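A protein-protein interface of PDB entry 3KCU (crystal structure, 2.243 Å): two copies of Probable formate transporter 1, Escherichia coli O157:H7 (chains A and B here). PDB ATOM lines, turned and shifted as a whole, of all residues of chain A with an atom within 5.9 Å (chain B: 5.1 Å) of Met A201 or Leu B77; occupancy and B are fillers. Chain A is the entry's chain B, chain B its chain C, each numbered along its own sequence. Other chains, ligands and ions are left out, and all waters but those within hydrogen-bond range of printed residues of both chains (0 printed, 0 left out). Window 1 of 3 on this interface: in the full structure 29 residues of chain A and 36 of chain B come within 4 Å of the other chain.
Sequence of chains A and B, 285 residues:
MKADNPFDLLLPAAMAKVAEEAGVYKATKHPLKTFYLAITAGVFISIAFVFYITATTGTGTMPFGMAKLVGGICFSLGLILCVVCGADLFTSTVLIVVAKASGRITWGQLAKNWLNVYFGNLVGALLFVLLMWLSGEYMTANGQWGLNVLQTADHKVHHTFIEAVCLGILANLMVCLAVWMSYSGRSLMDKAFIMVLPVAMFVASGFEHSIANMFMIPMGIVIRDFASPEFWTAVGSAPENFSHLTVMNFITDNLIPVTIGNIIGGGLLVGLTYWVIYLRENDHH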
ATOM      1  N   GLY A  72       1.716  36.139  -0.738  1.00  0.00           N
ATOM      2  CA  GLY A  72       0.665  35.153  -0.582  1.00  0.00           C
ATOM      3  C   GLY A  72      -0.565  35.795   0.022  1.00  0.00           C
ATOM      4  O   GLY A  72      -1.675  35.503  -0.390  1.00  0.00           O
ATOM      5  N   MET A 174      -5.515  23.359   0.175  1.00  0.00           N
ATOM      6  CA  MET A 174      -5.610  24.630   0.884  1.00  0.00           C
ATOM      7  C   MET A 174      -6.769  25.496   0.360  1.00  0.00           C
ATOM      8  O   MET A 174      -7.455  26.154   1.133  1.00  0.00           O
ATOM      9  CB  MET A 174      -4.276  25.398   0.813  1.00  0.00           C
ATOM     10  CG  MET A 174      -3.086  24.643   1.414  1.00  0.00           C
ATOM     11  SD  MET A 174      -3.471  23.845   3.001  1.00  0.00           S
ATOM     12  CE  MET A 174      -3.895  25.288   4.018  1.00  0.00           C
ATOM     13  N   MET A 181     -14.058  26.667   5.143  1.00  0.00           N
ATOM     14  CA  MET A 181     -14.121  27.565   6.298  1.00  0.00           C
ATOM     15  C   MET A 181     -14.959  28.818   6.006  1.00  0.00           C
ATOM     16  O   MET A 181     -15.776  29.243   6.819  1.00  0.00           O
ATOM     17  CB  MET A 181     -12.707  27.963   6.734  1.00  0.00           C
ATOM     18  CG  MET A 181     -11.865  26.779   7.227  1.00  0.00           C
ATOM     19  SD  MET A 181     -10.547  27.293   8.347  1.00  0.00           S
ATOM     20  CE  MET A 181      -9.309  27.913   7.183  1.00  0.00           C
ATOM     21  N   VAL A 196      -7.488  34.154   4.321  1.00  0.00           N
ATOM     22  CA  VAL A 196      -6.187  34.760   4.062  1.00  0.00           C
ATOM     23  C   VAL A 196      -5.020  33.777   4.349  1.00  0.00           C
ATOM     24  O   VAL A 196      -4.192  33.501   3.481  1.00  0.00           O
ATOM     25  CB  VAL A 196      -6.014  36.114   4.814  1.00  0.00           C
ATOM     26  CG1 VAL A 196      -4.620  36.715   4.560  1.00  0.00           C
ATOM     27  CG2 VAL A 196      -7.113  37.148   4.384  1.00  0.00           C
ATOM     28  N   LEU A 197      -4.981  33.239   5.561  1.00  0.00           N
ATOM     29  CA  LEU A 197      -3.904  32.356   5.992  1.00  0.00           C
ATOM     30  C   LEU A 197      -3.743  31.114   5.092  1.00  0.00           C
ATOM     31  O   LEU A 197      -2.646  30.853   4.584  1.00  0.00           O
ATOM     32  CB  LEU A 197      -4.119  31.960   7.461  1.00  0.00           C
ATOM     33  CG  LEU A 197      -3.321  32.592   8.625  1.00  0.00           C
ATOM     34  CD1 LEU A 197      -2.470  33.805   8.246  1.00  0.00           C
ATOM     35  CD2 LEU A 197      -4.188  32.885   9.848  1.00  0.00           C
ATOM     36  N   PRO A 198      -4.831  30.346   4.879  1.00  0.00           N
ATOM     37  CA  PRO A 198      -4.645  29.121   4.081  1.00  0.00           C
ATOM     38  C   PRO A 198      -4.266  29.417   2.633  1.00  0.00           C
ATOM     39  O   PRO A 198      -3.529  28.626   2.042  1.00  0.00           O
ATOM     40  CB  PRO A 198      -6.021  28.430   4.150  1.00  0.00           C
ATOM     41  CG  PRO A 198      -6.979  29.526   4.566  1.00  0.00           C
ATOM     42  CD  PRO A 198      -6.185  30.425   5.455  1.00  0.00           C
ATOM     43  N   VAL A 199      -4.759  30.522   2.072  1.00  0.00           N
ATOM     44  CA  VAL A 199      -4.345  30.909   0.726  1.00  0.00           C
ATOM     45  C   VAL A 199      -2.872  31.366   0.709  1.00  0.00           C
ATOM     46  O   VAL A 199      -2.084  30.902  -0.114  1.00  0.00           O
ATOM     47  CB  VAL A 199      -5.267  31.999   0.099  1.00  0.00           C
ATOM     48  CG1 VAL A 199      -4.710  32.459  -1.258  1.00  0.00           C
ATOM     49  CG2 VAL A 199      -6.675  31.447  -0.094  1.00  0.00           C
ATOM     50  N   ALA A 200      -2.499  32.257   1.622  1.00  0.00           N
ATOM     51  CA  ALA A 200      -1.113  32.733   1.648  1.00  0.00           C
ATOM     52  C   ALA A 200      -0.171  31.538   1.833  1.00  0.00           C
ATOM     53  O   ALA A 200       0.957  31.531   1.332  1.00  0.00           O
ATOM     54  CB  ALA A 200      -0.903  33.745   2.752  1.00  0.00           C
ATOM     55  N   MET A 201      -0.662  30.523   2.537  1.00  0.00           N
ATOM     56  CA  MET A 201       0.148  29.357   2.859  1.00  0.00           C
ATOM     57  C   MET A 201       0.522  28.610   1.578  1.00  0.00           C
ATOM     58  O   MET A 201       1.698  28.313   1.334  1.00  0.00           O
ATOM     59  CB  MET A 201      -0.579  28.459   3.883  1.00  0.00           C
ATOM     60  CG  MET A 201       0.224  27.230   4.338  1.00  0.00           C
ATOM     61  SD  MET A 201      -0.051  25.817   3.256  1.00  0.00           S
ATOM     62  CE  MET A 201       1.066  24.604   3.980  1.00  0.00           C
ATOM     63  N   PHE A 202      -0.470  28.338   0.744  1.00  0.00           N
ATOM     64  CA  PHE A 202      -0.217  27.588  -0.481  1.00  0.00           C
ATOM     65  C   PHE A 202       0.614  28.408  -1.472  1.00  0.00           C
ATOM     66  O   PHE A 202       1.557  27.908  -2.101  1.00  0.00           O
ATOM     67  CB  PHE A 202      -1.538  27.002  -1.052  1.00  0.00           C
ATOM     68  CG  PHE A 202      -2.110  27.725  -2.257  1.00  0.00           C
ATOM     69  CD1 PHE A 202      -1.452  27.707  -3.483  1.00  0.00           C
ATOM     70  CD2 PHE A 202      -3.360  28.347  -2.179  1.00  0.00           C
ATOM     71  CE1 PHE A 202      -1.974  28.342  -4.593  1.00  0.00           C
ATOM     72  CE2 PHE A 202      -3.917  28.977  -3.299  1.00  0.00           C
ATOM     73  CZ  PHE A 202      -3.230  28.983  -4.503  1.00  0.00           C
ATOM     74  N   VAL A 203       0.292  29.693  -1.563  1.00  0.00           N
ATOM     75  CA  VAL A 203       0.985  30.574  -2.473  1.00  0.00           C
ATOM     76  C   VAL A 203       2.438  30.825  -2.038  1.00  0.00           C
ATOM     77  O   VAL A 203       3.352  30.685  -2.853  1.00  0.00           O
ATOM     78  CB  VAL A 203       0.219  31.906  -2.638  1.00  0.00           C
ATOM     79  CG1 VAL A 203       1.030  32.905  -3.460  1.00  0.00           C
ATOM     80  CG2 VAL A 203      -1.233  31.648  -3.221  1.00  0.00           C
ATOM     81  N   ALA A 204       2.654  31.191  -0.773  1.00  0.00           N
ATOM     82  CA  ALA A 204       4.003  31.464  -0.293  1.00  0.00           C
ATOM     83  C   ALA A 204       4.893  30.221  -0.422  1.00  0.00           C
ATOM     84  O   ALA A 204       6.106  30.332  -0.641  1.00  0.00           O
ATOM     85  CB  ALA A 204       3.991  31.975   1.175  1.00  0.00           C
ATOM     86  N   SER A 205       4.276  29.051  -0.272  1.00  0.00           N
ATOM     87  CA  SER A 205       4.984  27.778  -0.318  1.00  0.00           C
ATOM     88  C   SER A 205       5.285  27.317  -1.739  1.00  0.00           C
ATOM     89  O   SER A 205       5.982  26.323  -1.912  1.00  0.00           O
ATOM     90  CB  SER A 205       4.199  26.672   0.429  1.00  0.00           C
ATOM     91  OG  SER A 205       4.166  26.905   1.839  1.00  0.00           O
ATOM     92  N   GLY A 206       4.769  28.024  -2.749  1.00  0.00           N
ATOM     93  CA  GLY A 206       4.992  27.628  -4.138  1.00  0.00           C
ATOM     94  C   GLY A 206       4.186  26.395  -4.565  1.00  0.00           C
ATOM     95  O   GLY A 206       4.563  25.679  -5.502  1.00  0.00           O
ATOM     96  N   PHE A 207       3.073  26.120  -3.883  1.00  0.00           N
ATOM     97  CA  PHE A 207       2.199  25.036  -4.346  1.00  0.00           C
ATOM     98  C   PHE A 207       1.543  25.440  -5.680  1.00  0.00           C
ATOM     99  O   PHE A 207       1.573  26.603  -6.067  1.00  0.00           O
ATOM    100  CB  PHE A 207       1.173  24.621  -3.287  1.00  0.00           C
ATOM    101  CG  PHE A 207       1.788  24.141  -1.996  1.00  0.00           C
ATOM    102  CD1 PHE A 207       3.129  23.754  -1.943  1.00  0.00           C
ATOM    103  CD2 PHE A 207       1.023  24.076  -0.832  1.00  0.00           C
ATOM    104  CE1 PHE A 207       3.701  23.314  -0.738  1.00  0.00           C
ATOM    105  CE2 PHE A 207       1.577  23.640   0.363  1.00  0.00           C
ATOM    106  CZ  PHE A 207       2.925  23.261   0.417  1.00  0.00           C
ATOM    107  N   ILE B  47       0.329  21.125   8.054  1.00  0.00           N
ATOM    108  CA  ILE B  47       0.125  22.328   7.263  1.00  0.00           C
ATOM    109  C   ILE B  47       0.700  23.534   8.010  1.00  0.00           C
ATOM    110  O   ILE B  47       1.462  24.307   7.453  1.00  0.00           O
ATOM    111  CB  ILE B  47      -1.371  22.544   6.947  1.00  0.00           C
ATOM    112  CG1 ILE B  47      -1.797  21.626   5.799  1.00  0.00           C
ATOM    113  CG2 ILE B  47      -1.658  24.039   6.618  1.00  0.00           C
ATOM    114  CD1 ILE B  47      -3.335  21.468   5.638  1.00  0.00           C
ATOM    115  N   ALA B  48       0.346  23.663   9.287  1.00  0.00           N
ATOM    116  CA  ALA B  48       0.867  24.729  10.140  1.00  0.00           C
ATOM    117  C   ALA B  48       2.409  24.789  10.198  1.00  0.00           C
ATOM    118  O   ALA B  48       2.994  25.858  10.045  1.00  0.00           O
ATOM    119  CB  ALA B  48       0.274  24.598  11.560  1.00  0.00           C
ATOM    120  N   VAL B  50       4.504  23.403   8.084  1.00  0.00           N
ATOM    121  CA  VAL B  50       4.969  23.717   6.739  1.00  0.00           C
ATOM    122  C   VAL B  50       4.937  25.253   6.486  1.00  0.00           C
ATOM    123  O   VAL B  50       5.888  25.819   5.933  1.00  0.00           O
ATOM    124  CB  VAL B  50       4.189  22.909   5.654  1.00  0.00           C
ATOM    125  CG1 VAL B  50       4.460  23.493   4.259  1.00  0.00           C
ATOM    126  CG2 VAL B  50       4.588  21.383   5.709  1.00  0.00           C
ATOM    127  N   PHE B  51       3.854  25.907   6.918  1.00  0.00           N
ATOM    128  CA  PHE B  51       3.676  27.368   6.769  1.00  0.00           C
ATOM    129  C   PHE B  51       4.791  28.082   7.527  1.00  0.00           C
ATOM    130  O   PHE B  51       5.463  28.982   7.002  1.00  0.00           O
ATOM    131  CB  PHE B  51       2.311  27.789   7.348  1.00  0.00           C
ATOM    132  CG  PHE B  51       1.787  29.100   6.822  1.00  0.00           C
ATOM    133  CD1 PHE B  51       2.526  29.866   5.923  1.00  0.00           C
ATOM    134  CD2 PHE B  51       0.542  29.569   7.231  1.00  0.00           C
ATOM    135  CE1 PHE B  51       2.035  31.075   5.443  1.00  0.00           C
ATOM    136  CE2 PHE B  51       0.041  30.779   6.757  1.00  0.00           C
ATOM    137  CZ  PHE B  51       0.791  31.542   5.869  1.00  0.00           C
ATOM    138  N   ILE B  73       2.656  33.190  13.905  1.00  0.00           N
ATOM    139  CA  ILE B  73       1.379  33.711  13.423  1.00  0.00           C
ATOM    140  C   ILE B  73       0.900  32.827  12.274  1.00  0.00           C
ATOM    141  O   ILE B  73      -0.275  32.471  12.181  1.00  0.00           O
ATOM    142  CB  ILE B  73       1.517  35.188  12.933  1.00  0.00           C
ATOM    143  CG1 ILE B  73       1.606  36.160  14.124  1.00  0.00           C
ATOM    144  CG2 ILE B  73       0.383  35.559  11.976  1.00  0.00           C
ATOM    145  CD1 ILE B  73       1.927  37.616  13.713  1.00  0.00           C
ATOM    146  N   CYS B  74       1.828  32.460  11.401  1.00  0.00           N
ATOM    147  CA  CYS B  74       1.495  31.592  10.276  1.00  0.00           C
ATOM    148  C   CYS B  74       1.065  30.207  10.766  1.00  0.00           C
ATOM    149  O   CYS B  74       0.117  29.609  10.235  1.00  0.00           O
ATOM    150  CB  CYS B  74       2.673  31.486   9.306  1.00  0.00           C
ATOM    151  SG  CYS B  74       3.012  33.035   8.412  1.00  0.00           S
ATOM    152  N   PHE B  75       1.751  29.726  11.800  1.00  0.00           N
ATOM    153  CA  PHE B  75       1.488  28.414  12.387  1.00  0.00           C
ATOM    154  C   PHE B  75       0.043  28.285  12.879  1.00  0.00           C
ATOM    155  O   PHE B  75      -0.530  27.192  12.868  1.00  0.00           O
ATOM    156  CB  PHE B  75       2.470  28.141  13.537  1.00  0.00           C
ATOM    157  CG  PHE B  75       2.420  26.725  14.074  1.00  0.00           C
ATOM    158  CD1 PHE B  75       3.366  25.785  13.683  1.00  0.00           C
ATOM    159  CD2 PHE B  75       1.434  26.340  14.973  1.00  0.00           C
ATOM    160  CE1 PHE B  75       3.335  24.479  14.186  1.00  0.00           C
ATOM    161  CE2 PHE B  75       1.389  25.038  15.483  1.00  0.00           C
ATOM    162  CZ  PHE B  75       2.346  24.104  15.086  1.00  0.00           C
ATOM    163  N   SER B  76      -0.542  29.400  13.306  1.00  0.00           N
ATOM    164  CA  SER B  76      -1.885  29.382  13.887  1.00  0.00           C
ATOM    165  C   SER B  76      -2.938  28.841  12.918  1.00  0.00           C
ATOM    166  O   SER B  76      -3.992  28.354  13.355  1.00  0.00           O
ATOM    167  CB  SER B  76      -2.289  30.775  14.416  1.00  0.00           C
ATOM    168  OG  SER B  76      -2.473  31.690  13.349  1.00  0.00           O
ATOM    169  N   LEU B  77      -2.665  28.946  11.614  1.00  0.00           N
ATOM    170  CA  LEU B  77      -3.492  28.289  10.594  1.00  0.00           C
ATOM    171  C   LEU B  77      -3.931  26.898  11.060  1.00  0.00           C
ATOM    172  O   LEU B  77      -5.093  26.540  10.945  1.00  0.00           O
ATOM    173  CB  LEU B  77      -2.705  28.088   9.296  1.00  0.00           C
ATOM    174  CG  LEU B  77      -3.438  28.196   7.947  1.00  0.00           C
ATOM    175  CD1 LEU B  77      -2.753  27.373   6.870  1.00  0.00           C
ATOM    176  CD2 LEU B  77      -4.942  27.895   8.018  1.00  0.00           C
ATOM    177  N   GLY B  78      -2.978  26.103  11.546  1.00  0.00           N
ATOM    178  CA  GLY B  78      -3.259  24.721  11.923  1.00  0.00           C
ATOM    179  C   GLY B  78      -4.316  24.568  13.002  1.00  0.00           C
ATOM    180  O   GLY B  78      -5.219  23.726  12.900  1.00  0.00           O
ATOM    181  N   LEU B  79      -4.206  25.374  14.052  1.00  0.00           N
ATOM    182  CA  LEU B  79      -5.202  25.337  15.110  1.00  0.00           C
ATOM    183  C   LEU B  79      -6.528  25.891  14.605  1.00  0.00           C
ATOM    184  O   LEU B  79      -7.593  25.413  15.005  1.00  0.00           O
ATOM    185  CB  LEU B  79      -4.734  26.091  16.358  1.00  0.00           C
ATOM    186  CG  LEU B  79      -5.425  25.635  17.646  1.00  0.00           C
ATOM    187  CD1 LEU B  79      -5.414  24.106  17.751  1.00  0.00           C
ATOM    188  CD2 LEU B  79      -4.811  26.271  18.893  1.00  0.00           C
ATOM    189  N   ILE B  80      -6.468  26.882  13.713  1.00  0.00           N
ATOM    190  CA  ILE B  80      -7.691  27.466  13.168  1.00  0.00           C
ATOM    191  C   ILE B  80      -8.438  26.418  12.338  1.00  0.00           C
ATOM    192  O   ILE B  80      -9.656  26.238  12.468  1.00  0.00           O
ATOM    193  CB  ILE B  80      -7.410  28.743  12.351  1.00  0.00           C
ATOM    194  CG1 ILE B  80      -7.002  29.888  13.295  1.00  0.00           C
ATOM    195  CG2 ILE B  80      -8.626  29.107  11.498  1.00  0.00           C
ATOM    196  CD1 ILE B  80      -6.330  31.127  12.565  1.00  0.00           C
ATOM    197  N   LEU B  81      -7.684  25.722  11.500  1.00  0.00           N
ATOM    198  CA  LEU B  81      -8.180  24.561  10.767  1.00  0.00           C
ATOM    199  C   LEU B  81      -8.862  23.532  11.693  1.00  0.00           C
ATOM    200  O   LEU B  81      -9.997  23.107  11.440  1.00  0.00           O
ATOM    201  CB  LEU B  81      -7.010  23.905  10.031  1.00  0.00           C
ATOM    202  CG  LEU B  81      -6.846  23.977   8.502  1.00  0.00           C
ATOM    203  CD1 LEU B  81      -7.825  24.900   7.786  1.00  0.00           C
ATOM    204  CD2 LEU B  81      -5.387  24.264   8.084  1.00  0.00           C
ATOM    205  N   CYS B  82      -8.178  23.139  12.768  1.00  0.00           N
ATOM    206  CA  CYS B  82      -8.718  22.117  13.675  1.00  0.00           C
ATOM    207  C   CYS B  82     -10.058  22.518  14.297  1.00  0.00           C
ATOM    208  O   CYS B  82     -11.005  21.728  14.311  1.00  0.00           O
ATOM    209  CB  CYS B  82      -7.720  21.763  14.791  1.00  0.00           C
ATOM    210  SG  CYS B  82      -6.276  20.836  14.252  1.00  0.00           S
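The side-chain hydroxyl (OG) of Ser A205 is in hydrogen-bond range of the backbone carbonyl oxygen (O) of Met A201.
Among the printed residues, merely in contact across the chains: Met A181 with Leu B81 (3.4 Å), Leu A197 with Phe B51 (3.5 Å), Met A201 with Phe B51 (3.5 Å), Met A201 with Ile B47 (3.5 Å), Met A174 with Ile B47 (3.6 Å), Met A201 with Val B50 (3.6 Å), Met A174 with Leu B77 (3.7 Å), Pro A198 with Leu B77 (3.8 Å), Met A201 with Leu B77 (3.9 Å), Leu A197 with Leu B77 (3.9 Å) and Leu A197 with Ile B80 (3.9 Å).
Of the printed residues of chain B, Met A181 touches Leu B81.
Printed residues of chain B within 4 Å of Leu A197: Phe B51 (3.5 Å), Leu B77 (3.9 Å) and Ile B80 (3.9 Å).
Of chain B, only Ile B47 (3.5 Å), Val B50 (3.6 Å), Phe B51 (3.5 Å) and Leu B77 (3.9 Å) come within 4 Å of Met A201.
Printed residues of chain A within 4 Å of Phe B51: Leu A197 (3.5 Å) and Met A201 (3.5 Å).
Cys B74 touches none of the printed residues of chain A.
Phe B75 touches none of the printed residues of chain A.
Of the printed residues of chain A, Leu B77 touches Met A174 (3.7 Å), Leu A197 (3.9 Å), Pro A198 (3.8 Å) and Met A201 (3.9 Å).
Printed residues of chain A within 4 Å of Ile B80: Leu A197 (3.9 Å).
The nearest printed residue of chain B that does not touch Met A201 is Ala B48 (5.4 Å).
Of the 15 printed residues of chain A, 5 touch a printed residue of chain B.
Hydrophobic or aromatic side chains of chain A within 4 Å of the printed part of chain B: Met A174, Met A181, Leu A197, Pro A198 and Met A201.
Printed residues of chain B that touch a printed residue of chain A: Ile B47, Val B50, Phe B51, Leu B77, Ile B80 and Leu B81.
Hydrophobic or aromatic side chains of chain B that line the printed part of chain A: Ile B47, Val B50, Phe B51, Leu B77, Ile B80 and Leu B81.
Among the printed residues, 11 pairs touch across the chains.
No position is printed for both chains.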
